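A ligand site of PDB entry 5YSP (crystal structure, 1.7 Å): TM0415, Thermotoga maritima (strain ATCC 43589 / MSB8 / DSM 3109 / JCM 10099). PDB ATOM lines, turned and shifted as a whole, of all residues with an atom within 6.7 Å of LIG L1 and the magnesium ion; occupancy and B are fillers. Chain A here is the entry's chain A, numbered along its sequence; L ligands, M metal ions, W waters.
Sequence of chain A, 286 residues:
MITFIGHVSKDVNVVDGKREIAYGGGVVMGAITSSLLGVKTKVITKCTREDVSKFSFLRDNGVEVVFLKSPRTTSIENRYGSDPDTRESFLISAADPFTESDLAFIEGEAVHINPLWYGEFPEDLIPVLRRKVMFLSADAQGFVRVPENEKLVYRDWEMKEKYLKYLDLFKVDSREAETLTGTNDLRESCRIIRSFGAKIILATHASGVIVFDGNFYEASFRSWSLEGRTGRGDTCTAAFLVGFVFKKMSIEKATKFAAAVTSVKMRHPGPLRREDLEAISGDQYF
An oxygen (O4) of LIG L1 sits at hydrogen-bond distance from the side-chain hydroxyl of Thr 204 (2.6 Å).
O5 of LIG L1 lies close to OD2 of Asp 173 (2.6 Å).
The side-chain amino group of Lys 171 is in salt-bridge range of an oxygen (O4) of LIG L1 (3.9 Å).
The backbone NH of Gly 233 lies within hydrogen-bond range of an oxygen (O2) of LIG L1, at 2.7 Å.
An oxygen (O4) of LIG L1 is in salt-bridge range of the guanidinium group (NE) of Arg 232 (2.7 Å).
O1 of LIG L1 is in hydrogen-bond range of N of Gly 231 (2.8 Å).
O2 of LIG L1 sits at hydrogen-bond distance from N of Asp 234 (2.9 Å).
An oxygen (O2) of LG2 L2 lies within hydrogen-bond range of the side-chain amide oxygen (OE1) of Gln 141 (2.8 Å).
The side-chain amino group (NZ) of Lys 171 is in hydrogen-bond range of the side-chain hydroxyl (OG1) of Thr 204.
The backbone carbonyl oxygen of Val 172 sits at hydrogen-bond distance from the backbone NH of Thr 204, 3.1 Å away.
The backbone carbonyl oxygen of Thr 204 sits at hydrogen-bond distance from the backbone NH of Ser 174.
The backbone NH (N) of Asp 173 is in hydrogen-bond range of the side-chain carboxylate (OE1) of Glu 176, 2.9 Å away.
O of His 205 lies within hydrogen-bond range of NH1 of Arg 232, at 3.4 Å.
The backbone carbonyl oxygen (O) of Gly 231 lies within hydrogen-bond range of the side-chain hydroxyl (OG1) of Thr 235.
The magnesium ion is bound by water W1 (1.8 Å), O3 of LIG L1 (2.0 Å), O6 of LIG L1 (2.0 Å), water W2 (2.1 Å), water W4 (2.2 Å) and water W3 (2.4 Å).
Residues that only touch LIG L1: Thr 230.
Within 4 Å of LIG L1: Lys 171, Asp 173, Thr 204, Thr 230, Gly 231, Arg 232, Gly 233 and Asp 234.
Water W4 lies within hydrogen-bond range of OD2 of Asp 139, O2 of LIG L1, OD1 of Asp 234 and NZ of Lys 171.
Water W2 lies within hydrogen-bond range of the side-chain carboxylate (OD1) of Asp 139 (3.0 Å) and the side-chain amide oxygen (OE1) of Gln 141 (3.4 Å).
Water W1 bridges the side-chain carboxylate (OE2) of Glu 176 (2.8 Å) and the side-chain carboxylate (OD2) of Asp 173 (3.0 Å).
Water W3 lies within hydrogen-bond range of the side-chain carboxylate (OE1) of Glu 176, the side-chain carboxylate (OD1) of Asp 139 and the side-chain amino group (NZ) of Lys 171.
Merely in contact with the magnesium ion: Lys 171 (3.8 Å).
Of the 20 residues printed, 1 comes within 4 Å of the magnesium ion.
O1 of LIG L1 is in hydrogen-bond range of O1 of LG2 L2 (2.7 Å).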
ATOM      1  N   GLY A  26     -20.063  38.121  25.919  1.00  0.00           N
ATOM      2  CA  GLY A  26     -21.014  37.065  25.625  1.00  0.00           C
ATOM      3  C   GLY A  26     -21.946  37.440  24.476  1.00  0.00           C
ATOM      4  O   GLY A  26     -22.206  36.618  23.568  1.00  0.00           O
ATOM      5  N   MET A  29     -20.274  37.143  20.966  1.00  0.00           N
ATOM      6  CA  MET A  29     -20.186  35.763  20.540  1.00  0.00           C
ATOM      7  C   MET A  29     -21.550  35.197  20.104  1.00  0.00           C
ATOM      8  O   MET A  29     -21.654  34.592  19.061  1.00  0.00           O
ATOM      9  CB  MET A  29     -19.578  34.899  21.633  1.00  0.00           C
ATOM     10  CG  MET A  29     -18.123  35.229  21.927  1.00  0.00           C
ATOM     11  SD  MET A  29     -17.077  34.550  20.625  1.00  0.00           S
ATOM     12  CE  MET A  29     -15.455  35.014  21.250  1.00  0.00           C
ATOM     13  N   ASP A 139     -27.906  33.065  30.763  1.00  0.00           N
ATOM     14  CA  ASP A 139     -26.625  32.444  31.043  1.00  0.00           C
ATOM     15  C   ASP A 139     -26.275  32.565  32.536  1.00  0.00           C
ATOM     16  O   ASP A 139     -26.247  33.654  33.084  1.00  0.00           O
ATOM     17  CB  ASP A 139     -25.538  33.123  30.211  1.00  0.00           C
ATOM     18  CG  ASP A 139     -24.274  32.292  30.137  1.00  0.00           C
ATOM     19  OD1 ASP A 139     -23.707  32.014  31.184  1.00  0.00           O
ATOM     20  OD2 ASP A 139     -23.855  31.904  29.027  1.00  0.00           O
ATOM     21  N   GLN A 141     -23.532  32.490  34.091  1.00  0.00           N
ATOM     22  CA  GLN A 141     -22.393  33.382  34.364  1.00  0.00           C
ATOM     23  C   GLN A 141     -22.865  34.692  35.009  1.00  0.00           C
ATOM     24  O   GLN A 141     -22.254  35.192  35.955  1.00  0.00           O
ATOM     25  CB  GLN A 141     -21.652  33.685  33.097  1.00  0.00           C
ATOM     26  CG  GLN A 141     -20.487  34.626  33.338  1.00  0.00           C
ATOM     27  CD  GLN A 141     -19.647  34.752  32.127  1.00  0.00           C
ATOM     28  OE1 GLN A 141     -18.646  34.064  32.028  1.00  0.00           O
ATOM     29  NE2 GLN A 141     -20.072  35.563  31.193  1.00  0.00           N
ATOM     30  N   LYS A 171     -28.430  28.336  30.563  1.00  0.00           N
ATOM     31  CA  LYS A 171     -27.117  27.912  30.104  1.00  0.00           C
ATOM     32  C   LYS A 171     -26.098  27.862  31.262  1.00  0.00           C
ATOM     33  O   LYS A 171     -25.951  28.800  32.010  1.00  0.00           O
ATOM     34  CB  LYS A 171     -26.627  28.888  29.012  1.00  0.00           C
ATOM     35  CG  LYS A 171     -25.142  28.833  28.711  1.00  0.00           C
ATOM     36  CD  LYS A 171     -24.748  27.562  28.017  1.00  0.00           C
ATOM     37  CE  LYS A 171     -23.290  27.585  27.569  1.00  0.00           C
ATOM     38  NZ  LYS A 171     -22.314  27.529  28.689  1.00  0.00           N
ATOM     39  N   VAL A 172     -25.413  26.724  31.409  1.00  0.00           N
ATOM     40  CA  VAL A 172     -24.369  26.552  32.390  1.00  0.00           C
ATOM     41  C   VAL A 172     -23.140  25.953  31.741  1.00  0.00           C
ATOM     42  O   VAL A 172     -23.227  25.335  30.680  1.00  0.00           O
ATOM     43  CB  VAL A 172     -24.763  25.587  33.556  1.00  0.00           C
ATOM     44  CG1 VAL A 172     -25.874  26.167  34.411  1.00  0.00           C
ATOM     45  CG2 VAL A 172     -25.165  24.199  33.047  1.00  0.00           C
ATOM     46  N   ASP A 173     -22.009  26.159  32.371  1.00  0.00           N
ATOM     47  CA  ASP A 173     -20.835  25.321  32.115  1.00  0.00           C
ATOM     48  C   ASP A 173     -20.538  24.494  33.368  1.00  0.00           C
ATOM     49  O   ASP A 173     -21.287  24.591  34.342  1.00  0.00           O
ATOM     50  CB  ASP A 173     -19.663  26.131  31.615  1.00  0.00           C
ATOM     51  CG  ASP A 173     -19.059  27.052  32.653  1.00  0.00           C
ATOM     52  OD1 ASP A 173     -19.418  27.045  33.859  1.00  0.00           O
ATOM     53  OD2 ASP A 173     -18.193  27.831  32.199  1.00  0.00           O
ATOM     54  N   SER A 174     -19.491  23.687  33.332  1.00  0.00           N
ATOM     55  CA  SER A 174     -19.186  22.810  34.484  1.00  0.00           C
ATOM     56  C   SER A 174     -19.081  23.529  35.834  1.00  0.00           C
ATOM     57  O   SER A 174     -19.694  23.140  36.866  1.00  0.00           O
ATOM     58  CB  SER A 174     -17.868  22.058  34.241  1.00  0.00           C
ATOM     59  OG  SER A 174     -17.948  21.320  33.039  1.00  0.00           O
ATOM     60  N   GLU A 176     -20.078  26.570  36.687  1.00  0.00           N
ATOM     61  CA  GLU A 176     -21.333  27.205  37.119  1.00  0.00           C
ATOM     62  C   GLU A 176     -22.321  26.175  37.678  1.00  0.00           C
ATOM     63  O   GLU A 176     -22.977  26.416  38.695  1.00  0.00           O
ATOM     64  CB  GLU A 176     -22.019  27.959  35.983  1.00  0.00           C
ATOM     65  CG  GLU A 176     -21.228  29.194  35.552  1.00  0.00           C
ATOM     66  CD  GLU A 176     -21.335  29.575  34.081  1.00  0.00           C
ATOM     67  OE1 GLU A 176     -22.069  28.936  33.292  1.00  0.00           O
ATOM     68  OE2 GLU A 176     -20.639  30.554  33.695  1.00  0.00           O
ATOM     69  N   THR A 204     -22.401  23.124  28.661  1.00  0.00           N
ATOM     70  CA  THR A 204     -21.196  22.891  27.895  1.00  0.00           C
ATOM     71  C   THR A 204     -20.106  22.416  28.848  1.00  0.00           C
ATOM     72  O   THR A 204     -20.060  22.776  30.020  1.00  0.00           O
ATOM     73  CB  THR A 204     -20.796  24.141  27.085  1.00  0.00           C
ATOM     74  OG1 THR A 204     -20.703  25.298  27.934  1.00  0.00           O
ATOM     75  CG2 THR A 204     -21.809  24.414  26.006  1.00  0.00           C
ATOM     76  N   HIS A 205     -19.264  21.532  28.336  1.00  0.00           N
ATOM     77  CA  HIS A 205     -18.072  21.070  29.036  1.00  0.00           C
ATOM     78  C   HIS A 205     -17.010  20.784  27.980  1.00  0.00           C
ATOM     79  O   HIS A 205     -17.267  20.940  26.790  1.00  0.00           O
ATOM     80  CB  HIS A 205     -18.410  19.826  29.869  1.00  0.00           C
ATOM     81  CG  HIS A 205     -18.906  18.660  29.066  1.00  0.00           C
ATOM     82  ND1 HIS A 205     -20.229  18.499  28.727  1.00  0.00           N
ATOM     83  CD2 HIS A 205     -18.250  17.626  28.503  1.00  0.00           C
ATOM     84  CE1 HIS A 205     -20.368  17.395  28.016  1.00  0.00           C
ATOM     85  NE2 HIS A 205     -19.179  16.848  27.856  1.00  0.00           N
ATOM     86  N   PHE A 221     -18.081  17.830  20.577  1.00  0.00           N
ATOM     87  CA  PHE A 221     -17.395  18.714  19.641  1.00  0.00           C
ATOM     88  C   PHE A 221     -16.449  17.900  18.759  1.00  0.00           C
ATOM     89  O   PHE A 221     -15.863  16.889  19.195  1.00  0.00           O
ATOM     90  CB  PHE A 221     -16.619  19.813  20.365  1.00  0.00           C
ATOM     91  CG  PHE A 221     -17.439  20.633  21.321  1.00  0.00           C
ATOM     92  CD1 PHE A 221     -18.650  21.201  20.947  1.00  0.00           C
ATOM     93  CD2 PHE A 221     -16.985  20.833  22.614  1.00  0.00           C
ATOM     94  CE1 PHE A 221     -19.382  21.949  21.839  1.00  0.00           C
ATOM     95  CE2 PHE A 221     -17.715  21.595  23.510  1.00  0.00           C
ATOM     96  CZ  PHE A 221     -18.909  22.150  23.118  1.00  0.00           C
ATOM     97  N   ARG A 229     -11.459  28.556  22.586  1.00  0.00           N
ATOM     98  CA  ARG A 229     -12.425  28.106  23.606  1.00  0.00           C
ATOM     99  C   ARG A 229     -13.299  29.244  24.184  1.00  0.00           C
ATOM    100  O   ARG A 229     -14.459  29.018  24.468  1.00  0.00           O
ATOM    101  CB  ARG A 229     -11.695  27.317  24.710  1.00  0.00           C
ATOM    102  N   THR A 230     -12.749  30.450  24.302  1.00  0.00           N
ATOM    103  CA  THR A 230     -13.544  31.594  24.808  1.00  0.00           C
ATOM    104  C   THR A 230     -14.704  31.866  23.854  1.00  0.00           C
ATOM    105  O   THR A 230     -14.523  31.910  22.637  1.00  0.00           O
ATOM    106  CB  THR A 230     -12.717  32.887  24.967  1.00  0.00           C
ATOM    107  OG1 THR A 230     -11.670  32.685  25.918  1.00  0.00           O
ATOM    108  CG2 THR A 230     -13.607  34.005  25.489  1.00  0.00           C
ATOM    109  N   GLY A 231     -15.908  31.960  24.410  1.00  0.00           N
ATOM    110  CA  GLY A 231     -17.108  32.040  23.598  1.00  0.00           C
ATOM    111  C   GLY A 231     -17.709  30.759  23.052  1.00  0.00           C
ATOM    112  O   GLY A 231     -18.714  30.819  22.342  1.00  0.00           O
ATOM    113  N   ARG A 232     -17.135  29.612  23.417  1.00  0.00           N
ATOM    114  CA  ARG A 232     -17.698  28.285  23.173  1.00  0.00           C
ATOM    115  C   ARG A 232     -19.151  28.232  23.592  1.00  0.00           C
ATOM    116  O   ARG A 232     -20.017  27.878  22.804  1.00  0.00           O
ATOM    117  CB  ARG A 232     -16.890  27.226  23.959  1.00  0.00           C
ATOM    118  CG  ARG A 232     -17.470  25.826  23.981  1.00  0.00           C
ATOM    119  CD  ARG A 232     -16.614  24.931  24.874  1.00  0.00           C
ATOM    120  NE  ARG A 232     -16.865  25.179  26.290  1.00  0.00           N
ATOM    121  CZ  ARG A 232     -16.205  24.585  27.276  1.00  0.00           C
ATOM    122  NH1 ARG A 232     -15.249  23.709  27.013  1.00  0.00           N
ATOM    123  NH2 ARG A 232     -16.502  24.849  28.537  1.00  0.00           N
ATOM    124  N   GLY A 233     -19.403  28.603  24.842  1.00  0.00           N
ATOM    125  CA  GLY A 233     -20.734  28.437  25.428  1.00  0.00           C
ATOM    126  C   GLY A 233     -21.731  29.390  24.800  1.00  0.00           C
ATOM    127  O   GLY A 233     -22.851  29.008  24.482  1.00  0.00           O
ATOM    128  N   ASP A 234     -21.303  30.629  24.600  1.00  0.00           N
ATOM    129  CA  ASP A 234     -22.180  31.643  23.978  1.00  0.00           C
ATOM    130  C   ASP A 234     -22.538  31.303  22.567  1.00  0.00           C
ATOM    131  O   ASP A 234     -23.700  31.445  22.157  1.00  0.00           O
ATOM    132  CB  ASP A 234     -21.556  33.017  24.117  1.00  0.00           C
ATOM    133  CG  ASP A 234     -21.546  33.461  25.558  1.00  0.00           C
ATOM    134  OD1 ASP A 234     -22.560  33.275  26.267  1.00  0.00           O
ATOM    135  OD2 ASP A 234     -20.521  33.897  26.044  1.00  0.00           O
ATOM    136  N   THR A 235     -21.566  30.773  21.830  1.00  0.00           N
ATOM    137  CA  THR A 235     -21.811  30.273  20.487  1.00  0.00           C
ATOM    138  C   THR A 235     -22.793  29.115  20.502  1.00  0.00           C
ATOM    139  O   THR A 235     -23.719  29.057  19.688  1.00  0.00           O
ATOM    140  CB  THR A 235     -20.466  29.849  19.837  1.00  0.00           C
ATOM    141  OG1 THR A 235     -19.580  30.986  19.789  1.00  0.00           O
ATOM    142  CG2 THR A 235     -20.660  29.302  18.445  1.00  0.00           C
ATOM    143  N   CYS A 236     -22.542  28.157  21.393  1.00  0.00           N
ATOM    144  CA  CYS A 236     -23.381  26.976  21.496  1.00  0.00           C
ATOM    145  C   CYS A 236     -24.840  27.343  21.832  1.00  0.00           C
ATOM    146  O   CYS A 236     -25.760  26.829  21.216  1.00  0.00           O
ATOM    147  CB  CYS A 236     -22.806  26.044  22.529  1.00  0.00           C
ATOM    148  SG  CYS A 236     -23.504  24.392  22.517  1.00  0.00           S
HETATM  149  O1  LIG L   1     -16.667  31.768  27.085  1.00  0.00           O
HETATM  150  P1  LIG L   1     -17.957  30.886  27.444  1.00  0.00           P
HETATM  151  O2  LIG L   1     -18.914  30.863  26.310  1.00  0.00           O
HETATM  152  O3  LIG L   1     -18.692  31.469  28.761  1.00  0.00           O
HETATM  153  C1  LIG L   1     -17.279  29.221  27.727  1.00  0.00           C
HETATM  154  P2  LIG L   1     -18.440  27.994  28.412  1.00  0.00           P
HETATM  155  O4  LIG L   1     -18.671  26.896  27.442  1.00  0.00           O
HETATM  156  O5  LIG L   1     -17.615  27.402  29.668  1.00  0.00           O
HETATM  157  O6  LIG L   1     -19.816  28.603  28.934  1.00  0.00           O
HETATM  158  C1  LG2 L   2     -16.293  34.962  28.252  1.00  0.00           C
HETATM  159  C2  LG2 L   2     -15.928  35.116  29.725  1.00  0.00           C
HETATM  160  C3  LG2 L   2     -14.688  35.987  29.845  1.00  0.00           C
HETATM  161  C4  LG2 L   2     -14.948  37.365  29.222  1.00  0.00           C
HETATM  162  C5  LG2 L   2     -15.379  37.234  27.756  1.00  0.00           C
HETATM  163  C6  LG2 L   2     -16.563  36.294  27.552  1.00  0.00           C
HETATM  164  O1  LG2 L   2     -17.456  34.143  28.115  1.00  0.00           O
HETATM  165  O2  LG2 L   2     -16.995  35.680  30.501  1.00  0.00           O
HETATM  166  O3  LG2 L   2     -14.299  36.134  31.214  1.00  0.00           O
HETATM  167  O4  LG2 L   2     -13.778  38.168  29.333  1.00  0.00           O
HETATM  168  O5  LG2 L   2     -15.777  38.524  27.272  1.00  0.00           O
HETATM  169  O6  LG2 L   2     -16.825  36.128  26.155  1.00  0.00           O
HETATM  170 MG    MG M   1     -20.155  30.457  29.710  1.00  0.00          MG
HETATM  171  O   HOH W   1     -19.256  30.427  31.268  1.00  0.00           O
HETATM  172  O   HOH W   2     -20.903  32.402  30.112  1.00  0.00           O
HETATM  173  O   HOH W   3     -22.214  29.697  30.751  1.00  0.00           O
HETATM  174  O   HOH W   4     -21.444  30.668  27.910  1.00  0.00           O
